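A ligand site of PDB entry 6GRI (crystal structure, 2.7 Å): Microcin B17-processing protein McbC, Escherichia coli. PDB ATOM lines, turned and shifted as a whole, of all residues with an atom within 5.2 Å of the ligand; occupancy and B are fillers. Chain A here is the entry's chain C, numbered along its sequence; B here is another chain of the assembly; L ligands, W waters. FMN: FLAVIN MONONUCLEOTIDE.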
ATOM      1  N   ARG A  82       7.217 -19.369  -0.800  1.00  0.00           N
ATOM      2  CA  ARG A  82       7.505 -20.221   0.365  1.00  0.00           C
ATOM      3  C   ARG A  82       6.634 -19.701   1.489  1.00  0.00           C
ATOM      4  O   ARG A  82       6.546 -18.486   1.690  1.00  0.00           O
ATOM      5  CB  ARG A  82       8.987 -20.116   0.746  1.00  0.00           C
ATOM      6  CG  ARG A  82       9.420 -20.916   1.969  1.00  0.00           C
ATOM      7  CD  ARG A  82      10.918 -20.766   2.218  1.00  0.00           C
ATOM      8  NE  ARG A  82      11.297 -19.369   2.432  1.00  0.00           N
ATOM      9  CZ  ARG A  82      11.297 -18.728   3.612  1.00  0.00           C
ATOM     10  NH1 ARG A  82      10.952 -19.330   4.746  1.00  0.00           N
ATOM     11  NH2 ARG A  82      11.655 -17.437   3.642  1.00  0.00           N
ATOM     12  N   LEU A  83       5.971 -20.612   2.205  1.00  0.00           N
ATOM     13  CA  LEU A  83       5.057 -20.190   3.282  1.00  0.00           C
ATOM     14  C   LEU A  83       5.821 -19.494   4.393  1.00  0.00           C
ATOM     15  O   LEU A  83       7.020 -19.717   4.544  1.00  0.00           O
ATOM     16  CB  LEU A  83       4.269 -21.373   3.862  1.00  0.00           C
ATOM     17  CG  LEU A  83       3.158 -21.890   2.943  1.00  0.00           C
ATOM     18  CD1 LEU A  83       2.850 -23.347   3.261  1.00  0.00           C
ATOM     19  CD2 LEU A  83       1.901 -21.025   3.044  1.00  0.00           C
ATOM     20  N   PRO A  84       5.135 -18.615   5.155  1.00  0.00           N
ATOM     21  CA  PRO A  84       5.758 -18.101   6.373  1.00  0.00           C
ATOM     22  C   PRO A  84       6.244 -19.244   7.261  1.00  0.00           C
ATOM     23  O   PRO A  84       5.575 -20.260   7.373  1.00  0.00           O
ATOM     24  CB  PRO A  84       4.609 -17.336   7.040  1.00  0.00           C
ATOM     25  CG  PRO A  84       3.788 -16.857   5.901  1.00  0.00           C
ATOM     26  CD  PRO A  84       3.859 -17.941   4.864  1.00  0.00           C
ATOM     27  N   SER A  85       7.426 -19.084   7.844  1.00  0.00           N
ATOM     28  CA  SER A  85       7.992 -20.129   8.707  1.00  0.00           C
ATOM     29  C   SER A  85       7.192 -20.216   9.998  1.00  0.00           C
ATOM     30  O   SER A  85       7.051 -19.224  10.717  1.00  0.00           O
ATOM     31  CB  SER A  85       9.468 -19.877   8.971  1.00  0.00           C
ATOM     32  OG  SER A  85      10.221 -20.198   7.822  1.00  0.00           O
ATOM     33  N   ILE A  87       5.514 -20.556  13.511  1.00  0.00           N
ATOM     34  CA  ILE A  87       5.911 -20.235  14.876  1.00  0.00           C
ATOM     35  C   ILE A  87       4.688 -20.484  15.723  1.00  0.00           C
ATOM     36  O   ILE A  87       3.587 -20.571  15.177  1.00  0.00           O
ATOM     37  CB  ILE A  87       6.424 -18.776  14.979  1.00  0.00           C
ATOM     38  CG1 ILE A  87       7.153 -18.526  16.318  1.00  0.00           C
ATOM     39  CG2 ILE A  87       5.293 -17.766  14.773  1.00  0.00           C
ATOM     40  CD1 ILE A  87       8.326 -19.459  16.597  1.00  0.00           C
ATOM     41  N   ASP A 178      13.679 -20.120  24.146  1.00  0.00           N
ATOM     42  CA  ASP A 178      12.526 -19.465  23.504  1.00  0.00           C
ATOM     43  C   ASP A 178      11.348 -20.415  23.234  1.00  0.00           C
ATOM     44  O   ASP A 178      10.588 -20.220  22.269  1.00  0.00           O
ATOM     45  CB  ASP A 178      13.026 -18.808  22.213  1.00  0.00           C
ATOM     46  CG  ASP A 178      12.026 -17.823  21.590  1.00  0.00           C
ATOM     47  OD1 ASP A 178      11.186 -17.239  22.303  1.00  0.00           O
ATOM     48  OD2 ASP A 178      12.109 -17.646  20.357  1.00  0.00           O
ATOM     49  N   ARG A 181       7.508 -19.008  22.907  1.00  0.00           N
ATOM     50  CA  ARG A 181       7.118 -18.535  21.575  1.00  0.00           C
ATOM     51  C   ARG A 181       7.043 -19.675  20.555  1.00  0.00           C
ATOM     52  O   ARG A 181       6.188 -19.663  19.669  1.00  0.00           O
ATOM     53  CB  ARG A 181       8.099 -17.464  21.077  1.00  0.00           C
ATOM     54  CG  ARG A 181       7.886 -16.997  19.652  1.00  0.00           C
ATOM     55  CD  ARG A 181       8.824 -15.856  19.319  1.00  0.00           C
ATOM     56  NE  ARG A 181       9.218 -15.872  17.917  1.00  0.00           N
ATOM     57  CZ  ARG A 181      10.163 -16.653  17.393  1.00  0.00           C
ATOM     58  NH1 ARG A 181      10.850 -17.511  18.140  1.00  0.00           N
ATOM     59  NH2 ARG A 181      10.416 -16.591  16.097  1.00  0.00           N
ATOM     60  N   TYR A 218      18.143 -29.075   4.770  1.00  0.00           N
ATOM     61  CA  TYR A 218      16.996 -28.420   5.419  1.00  0.00           C
ATOM     62  C   TYR A 218      16.124 -27.653   4.451  1.00  0.00           C
ATOM     63  O   TYR A 218      14.942 -27.443   4.730  1.00  0.00           O
ATOM     64  CB  TYR A 218      17.372 -27.580   6.665  1.00  0.00           C
ATOM     65  CG  TYR A 218      18.056 -26.229   6.502  1.00  0.00           C
ATOM     66  CD1 TYR A 218      17.502 -25.214   5.705  1.00  0.00           C
ATOM     67  CD2 TYR A 218      19.201 -25.925   7.250  1.00  0.00           C
ATOM     68  CE1 TYR A 218      18.114 -23.967   5.594  1.00  0.00           C
ATOM     69  CE2 TYR A 218      19.813 -24.678   7.139  1.00  0.00           C
ATOM     70  CZ  TYR A 218      19.264 -23.709   6.315  1.00  0.00           C
ATOM     71  OH  TYR A 218      19.852 -22.468   6.187  1.00  0.00           O
ATOM     72  N   ARG A 233      10.099 -24.559  10.819  1.00  0.00           N
ATOM     73  CA  ARG A 233      11.000 -23.502  11.220  1.00  0.00           C
ATOM     74  C   ARG A 233      12.383 -24.057  11.527  1.00  0.00           C
ATOM     75  O   ARG A 233      12.557 -24.810  12.500  1.00  0.00           O
ATOM     76  CB  ARG A 233      10.456 -22.786  12.447  1.00  0.00           C
ATOM     77  CG  ARG A 233      11.327 -21.650  12.973  1.00  0.00           C
ATOM     78  CD  ARG A 233      10.557 -20.775  13.949  1.00  0.00           C
ATOM     79  NE  ARG A 233       9.778 -19.774  13.232  1.00  0.00           N
ATOM     80  CZ  ARG A 233      10.192 -18.553  12.896  1.00  0.00           C
ATOM     81  NH1 ARG A 233      11.411 -18.115  13.235  1.00  0.00           N
ATOM     82  NH2 ARG A 233       9.383 -17.747  12.220  1.00  0.00           N
ATOM     83  N   VAL A 234      13.359 -23.688  10.692  1.00  0.00           N
ATOM     84  CA  VAL A 234      14.777 -23.865  11.014  1.00  0.00           C
ATOM     85  C   VAL A 234      15.064 -23.087  12.304  1.00  0.00           C
ATOM     86  O   VAL A 234      14.529 -21.992  12.479  1.00  0.00           O
ATOM     87  CB  VAL A 234      15.675 -23.352   9.880  1.00  0.00           C
ATOM     88  CG1 VAL A 234      17.129 -23.355  10.320  1.00  0.00           C
ATOM     89  CG2 VAL A 234      15.503 -24.213   8.650  1.00  0.00           C
ATOM     90  N   TRP A 235      15.876 -23.661  13.182  1.00  0.00           N
ATOM     91  CA  TRP A 235      16.029 -23.156  14.550  1.00  0.00           C
ATOM     92  C   TRP A 235      17.460 -23.274  15.047  1.00  0.00           C
ATOM     93  O   TRP A 235      18.059 -24.337  14.965  1.00  0.00           O
ATOM     94  CB  TRP A 235      15.120 -23.930  15.485  1.00  0.00           C
ATOM     95  CG  TRP A 235      14.994 -23.381  16.864  1.00  0.00           C
ATOM     96  CD1 TRP A 235      15.787 -23.659  17.936  1.00  0.00           C
ATOM     97  CD2 TRP A 235      13.959 -22.525  17.350  1.00  0.00           C
ATOM     98  NE1 TRP A 235      15.331 -23.001  19.055  1.00  0.00           N
ATOM     99  CE2 TRP A 235      14.203 -22.308  18.723  1.00  0.00           C
ATOM    100  CE3 TRP A 235      12.855 -21.912  16.758  1.00  0.00           C
ATOM    101  CZ2 TRP A 235      13.387 -21.500  19.502  1.00  0.00           C
ATOM    102  CZ3 TRP A 235      12.031 -21.114  17.552  1.00  0.00           C
ATOM    103  CH2 TRP A 235      12.303 -20.910  18.906  1.00  0.00           C
ATOM    104  N   ALA A 236      17.997 -22.174  15.569  1.00  0.00           N
ATOM    105  CA  ALA A 236      19.376 -22.114  16.023  1.00  0.00           C
ATOM    106  C   ALA A 236      19.496 -21.868  17.532  1.00  0.00           C
ATOM    107  O   ALA A 236      20.580 -22.013  18.076  1.00  0.00           O
ATOM    108  CB  ALA A 236      20.132 -21.056  15.229  1.00  0.00           C
ATOM    109  N   GLY A 237      18.403 -21.516  18.209  1.00  0.00           N
ATOM    110  CA  GLY A 237      18.436 -21.255  19.657  1.00  0.00           C
ATOM    111  C   GLY A 237      18.321 -22.503  20.523  1.00  0.00           C
ATOM    112  O   GLY A 237      17.271 -22.764  21.102  1.00  0.00           O
ATOM    113  N   ILE A 258      22.209 -27.695  13.148  1.00  0.00           N
ATOM    114  CA  ILE A 258      20.940 -27.007  13.078  1.00  0.00           C
ATOM    115  C   ILE A 258      19.749 -27.933  13.414  1.00  0.00           C
ATOM    116  O   ILE A 258      19.723 -29.109  13.022  1.00  0.00           O
ATOM    117  CB  ILE A 258      20.789 -26.384  11.668  1.00  0.00           C
ATOM    118  CG1 ILE A 258      19.681 -25.332  11.630  1.00  0.00           C
ATOM    119  CG2 ILE A 258      20.603 -27.458  10.606  1.00  0.00           C
ATOM    120  CD1 ILE A 258      20.082 -24.023  12.294  1.00  0.00           C
ATOM    121  N   ARG B 117       9.824 -11.564   1.263  1.00  0.00           N
ATOM    122  CA  ARG B 117      10.050 -12.970   1.596  1.00  0.00           C
ATOM    123  C   ARG B 117      10.700 -13.685   0.413  1.00  0.00           C
ATOM    124  O   ARG B 117      10.096 -13.778  -0.641  1.00  0.00           O
ATOM    125  CB  ARG B 117       8.752 -13.677   1.992  1.00  0.00           C
ATOM    126  CG  ARG B 117       8.912 -15.197   2.101  1.00  0.00           C
ATOM    127  CD  ARG B 117       7.759 -15.888   2.804  1.00  0.00           C
ATOM    128  NE  ARG B 117       7.707 -15.582   4.235  1.00  0.00           N
ATOM    129  CZ  ARG B 117       6.871 -14.712   4.822  1.00  0.00           C
ATOM    130  NH1 ARG B 117       5.978 -14.011   4.125  1.00  0.00           N
ATOM    131  NH2 ARG B 117       6.940 -14.551   6.145  1.00  0.00           N
ATOM    132  N   PRO B 121      15.007 -19.647   3.755  1.00  0.00           N
ATOM    133  CA  PRO B 121      15.059 -18.900   5.004  1.00  0.00           C
ATOM    134  C   PRO B 121      16.491 -18.539   5.419  1.00  0.00           C
ATOM    135  O   PRO B 121      17.473 -19.153   4.944  1.00  0.00           O
ATOM    136  CB  PRO B 121      14.431 -19.875   5.997  1.00  0.00           C
ATOM    137  CG  PRO B 121      14.809 -21.223   5.473  1.00  0.00           C
ATOM    138  CD  PRO B 121      15.055 -21.099   4.004  1.00  0.00           C
ATOM    139  N   SER B 122      16.594 -17.581   6.336  1.00  0.00           N
ATOM    140  CA  SER B 122      17.851 -17.016   6.791  1.00  0.00           C
ATOM    141  C   SER B 122      17.789 -16.676   8.278  1.00  0.00           C
ATOM    142  O   SER B 122      16.796 -16.133   8.740  1.00  0.00           O
ATOM    143  CB  SER B 122      18.137 -15.743   5.991  1.00  0.00           C
ATOM    144  OG  SER B 122      19.331 -15.096   6.400  1.00  0.00           O
ATOM    145  N   GLY B 123      18.830 -17.001   9.021  1.00  0.00           N
ATOM    146  CA  GLY B 123      18.919 -16.621  10.417  1.00  0.00           C
ATOM    147  C   GLY B 123      18.773 -15.119  10.656  1.00  0.00           C
ATOM    148  O   GLY B 123      19.556 -14.328  10.134  1.00  0.00           O
ATOM    149  N   GLY B 124      17.769 -14.734  11.427  1.00  0.00           N
ATOM    150  CA  GLY B 124      17.493 -13.317  11.686  1.00  0.00           C
ATOM    151  C   GLY B 124      17.015 -12.497  10.504  1.00  0.00           C
ATOM    152  O   GLY B 124      17.001 -11.266  10.573  1.00  0.00           O
ATOM    153  N   ALA B 125      16.605 -13.169   9.427  1.00  0.00           N
ATOM    154  CA  ALA B 125      16.286 -12.541   8.153  1.00  0.00           C
ATOM    155  C   ALA B 125      17.408 -11.596   7.675  1.00  0.00           C
ATOM    156  O   ALA B 125      17.141 -10.547   7.077  1.00  0.00           O
ATOM    157  CB  ALA B 125      14.950 -11.829   8.245  1.00  0.00           C
ATOM    158  N   TYR B 127      20.216 -12.520   5.635  1.00  0.00           N
ATOM    159  CA  TYR B 127      20.627 -12.787   4.262  1.00  0.00           C
ATOM    160  C   TYR B 127      22.045 -12.279   3.959  1.00  0.00           C
ATOM    161  O   TYR B 127      22.211 -11.360   3.155  1.00  0.00           O
ATOM    162  CB  TYR B 127      19.575 -12.227   3.288  1.00  0.00           C
ATOM    163  CG  TYR B 127      18.268 -12.969   3.422  1.00  0.00           C
ATOM    164  CD1 TYR B 127      18.073 -14.163   2.759  1.00  0.00           C
ATOM    165  CD2 TYR B 127      17.245 -12.494   4.241  1.00  0.00           C
ATOM    166  CE1 TYR B 127      16.908 -14.882   2.892  1.00  0.00           C
ATOM    167  CE2 TYR B 127      16.064 -13.210   4.380  1.00  0.00           C
ATOM    168  CZ  TYR B 127      15.902 -14.413   3.691  1.00  0.00           C
ATOM    169  OH  TYR B 127      14.746 -15.172   3.789  1.00  0.00           O
ATOM    170  N   MET B 209      25.595 -20.374  10.342  1.00  0.00           N
ATOM    171  CA  MET B 209      24.303 -20.022   9.757  1.00  0.00           C
ATOM    172  C   MET B 209      24.448 -19.478   8.323  1.00  0.00           C
ATOM    173  O   MET B 209      23.639 -19.817   7.457  1.00  0.00           O
ATOM    174  CB  MET B 209      23.589 -19.000  10.636  1.00  0.00           C
ATOM    175  CG  MET B 209      23.123 -19.547  11.963  1.00  0.00           C
ATOM    176  SD  MET B 209      22.761 -18.226  13.142  1.00  0.00           S
ATOM    177  CE  MET B 209      21.018 -17.946  12.897  1.00  0.00           C
ATOM    178  N   MET B 212      25.473 -22.520   5.920  1.00  0.00           N
ATOM    179  CA  MET B 212      24.297 -23.355   5.660  1.00  0.00           C
ATOM    180  C   MET B 212      23.292 -22.658   4.732  1.00  0.00           C
ATOM    181  O   MET B 212      22.721 -23.293   3.841  1.00  0.00           O
ATOM    182  CB  MET B 212      23.592 -23.751   6.958  1.00  0.00           C
ATOM    183  CG  MET B 212      24.418 -24.678   7.851  1.00  0.00           C
ATOM    184  SD  MET B 212      23.537 -25.121   9.352  1.00  0.00           S
ATOM    185  CE  MET B 212      23.409 -23.560  10.210  1.00  0.00           C
HETATM  186  N1  FMN L   1      13.884 -18.576  13.957  1.00  0.00           N
HETATM  187  C2  FMN L   1      13.774 -18.482  15.313  1.00  0.00           C
HETATM  188  O2  FMN L   1      12.706 -18.063  15.786  1.00  0.00           O
HETATM  189  N3  FMN L   1      14.782 -18.822  16.146  1.00  0.00           N
HETATM  190  C4  FMN L   1      15.962 -19.277  15.669  1.00  0.00           C
HETATM  191  O4  FMN L   1      16.888 -19.578  16.445  1.00  0.00           O
HETATM  192  C4A FMN L   1      16.154 -19.407  14.205  1.00  0.00           C
HETATM  193  N5  FMN L   1      17.318 -19.864  13.679  1.00  0.00           N
HETATM  194  C5A FMN L   1      17.473 -19.975  12.336  1.00  0.00           C
HETATM  195  C6  FMN L   1      18.685 -20.453  11.836  1.00  0.00           C
HETATM  196  C7  FMN L   1      18.902 -20.595  10.468  1.00  0.00           C
HETATM  197  C7M FMN L   1      20.213 -21.108   9.944  1.00  0.00           C
HETATM  198  C8  FMN L   1      17.808 -20.223   9.531  1.00  0.00           C
HETATM  199  C8M FMN L   1      18.005 -20.366   8.048  1.00  0.00           C
HETATM  200  C9  FMN L   1      16.592 -19.756  10.023  1.00  0.00           C
HETATM  201  C9A FMN L   1      16.371 -19.606  11.394  1.00  0.00           C
HETATM  202  N10 FMN L   1      15.129 -19.123  11.935  1.00  0.00           N
HETATM  203  C10 FMN L   1      15.007 -19.019  13.341  1.00  0.00           C
HETATM  204  C1' FMN L   1      13.998 -18.736  11.066  1.00  0.00           C
HETATM  205  C2' FMN L   1      14.227 -17.322  10.535  1.00  0.00           C
HETATM  206  O2' FMN L   1      14.076 -16.402  11.620  1.00  0.00           O
HETATM  207  C3' FMN L   1      13.278 -16.984   9.381  1.00  0.00           C
HETATM  208  O3' FMN L   1      13.631 -17.797   8.251  1.00  0.00           O
HETATM  209  C4' FMN L   1      13.342 -15.506   8.960  1.00  0.00           C
HETATM  210  O4' FMN L   1      12.858 -14.665  10.000  1.00  0.00           O
HETATM  211  C5' FMN L   1      12.525 -15.216   7.701  1.00  0.00           C
HETATM  212  O5' FMN L   1      11.144 -15.505   7.944  1.00  0.00           O
HETATM  213  P   FMN L   1      10.328 -16.573   7.061  1.00  0.00           P
HETATM  214  O1P FMN L   1      11.178 -17.825   7.095  1.00  0.00           O
HETATM  215  O2P FMN L   1       9.026 -16.666   7.824  1.00  0.00           O
HETATM  216  O3P FMN L   1      10.234 -15.989   5.671  1.00  0.00           O
HETATM  217  O   HOH W   1      18.930 -17.779  16.650  1.00  0.00           O
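NH1 of Arg 233 lies within hydrogen-bond range of N1 of the ligand, 2.6 Å away.
O2P of the ligand sits at hydrogen-bond distance from N of Ser 85.
An oxygen (O1P) of the ligand sits at hydrogen-bond distance from the side-chain hydroxyl (OG) of Ser 85, 2.7 Å away.
The guanidinium group (NH2) of Arg 181 lies within hydrogen-bond range of an oxygen (O2) of the ligand, 2.7 Å away.
The guanidinium group (NH1) of Arg 82 is in salt-bridge range of an oxygen (O1P) of the ligand, at 2.8 Å.
An oxygen (O3P) of the ligand is in salt-bridge range of the guanidinium group of Arg 117 of chain B (2.9 Å).
N of Ala 236 is in hydrogen-bond range of O4 of the ligand (3.0 Å).
The backbone NH (N) of Gly 237 sits at hydrogen-bond distance from an oxygen (O4) of the ligand (3.0 Å).
The backbone carbonyl oxygen (O) of Ser 85 lies within hydrogen-bond range of the guanidinium group (NH2) of Arg 233 (3.1 Å).
OG of Ser 85 lies within hydrogen-bond range of NH1 of Arg 82.
The guanidinium group of Arg 181 is in salt-bridge range of the side-chain carboxylate of Asp 178 (2.6 Å).
The backbone carbonyl oxygen of Gly 237 is in hydrogen-bond range of the indole nitrogen of Trp 235 (2.8 Å).
The side-chain hydroxyl (OG) of Ser 122 of chain B lies within hydrogen-bond range of the backbone NH (N) of Tyr 127 of chain B (2.8 Å).
O of Val 234 sits close to N10 of the ligand, at 3.0 Å.
Pro 84 touches the ligand.
OH of Tyr 218 touches C8M of the ligand, at 3.4 Å.
CZ3 of Trp 235 touches O2 of the ligand (3.6 Å).
Ile 258 touches the ligand (CD1 to C7M, 3.7 Å).
CB of Pro 121 of chain B touches O3' of the ligand (3.2 Å).
Ser 122 of chain B touches the ligand.
Gly 123 of chain B touches the ligand (N to C8, 3.4 Å).
Ala 125 of chain B touches the ligand.
CE of Met 209 of chain B touches C6 of the ligand, 3.6 Å away.
17 residues have an atom within 4 Å of the ligand: Arg 82, Pro 84, Ser 85, Arg 181, Tyr 218, Arg 233, Val 234, Trp 235, Ala 236, Gly 237, Ile 258, Arg 117 of chain B, Pro 121 of chain B, Ser 122 of chain B, Gly 123 of chain B, Ala 125 of chain B and Met 209 of chain B.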
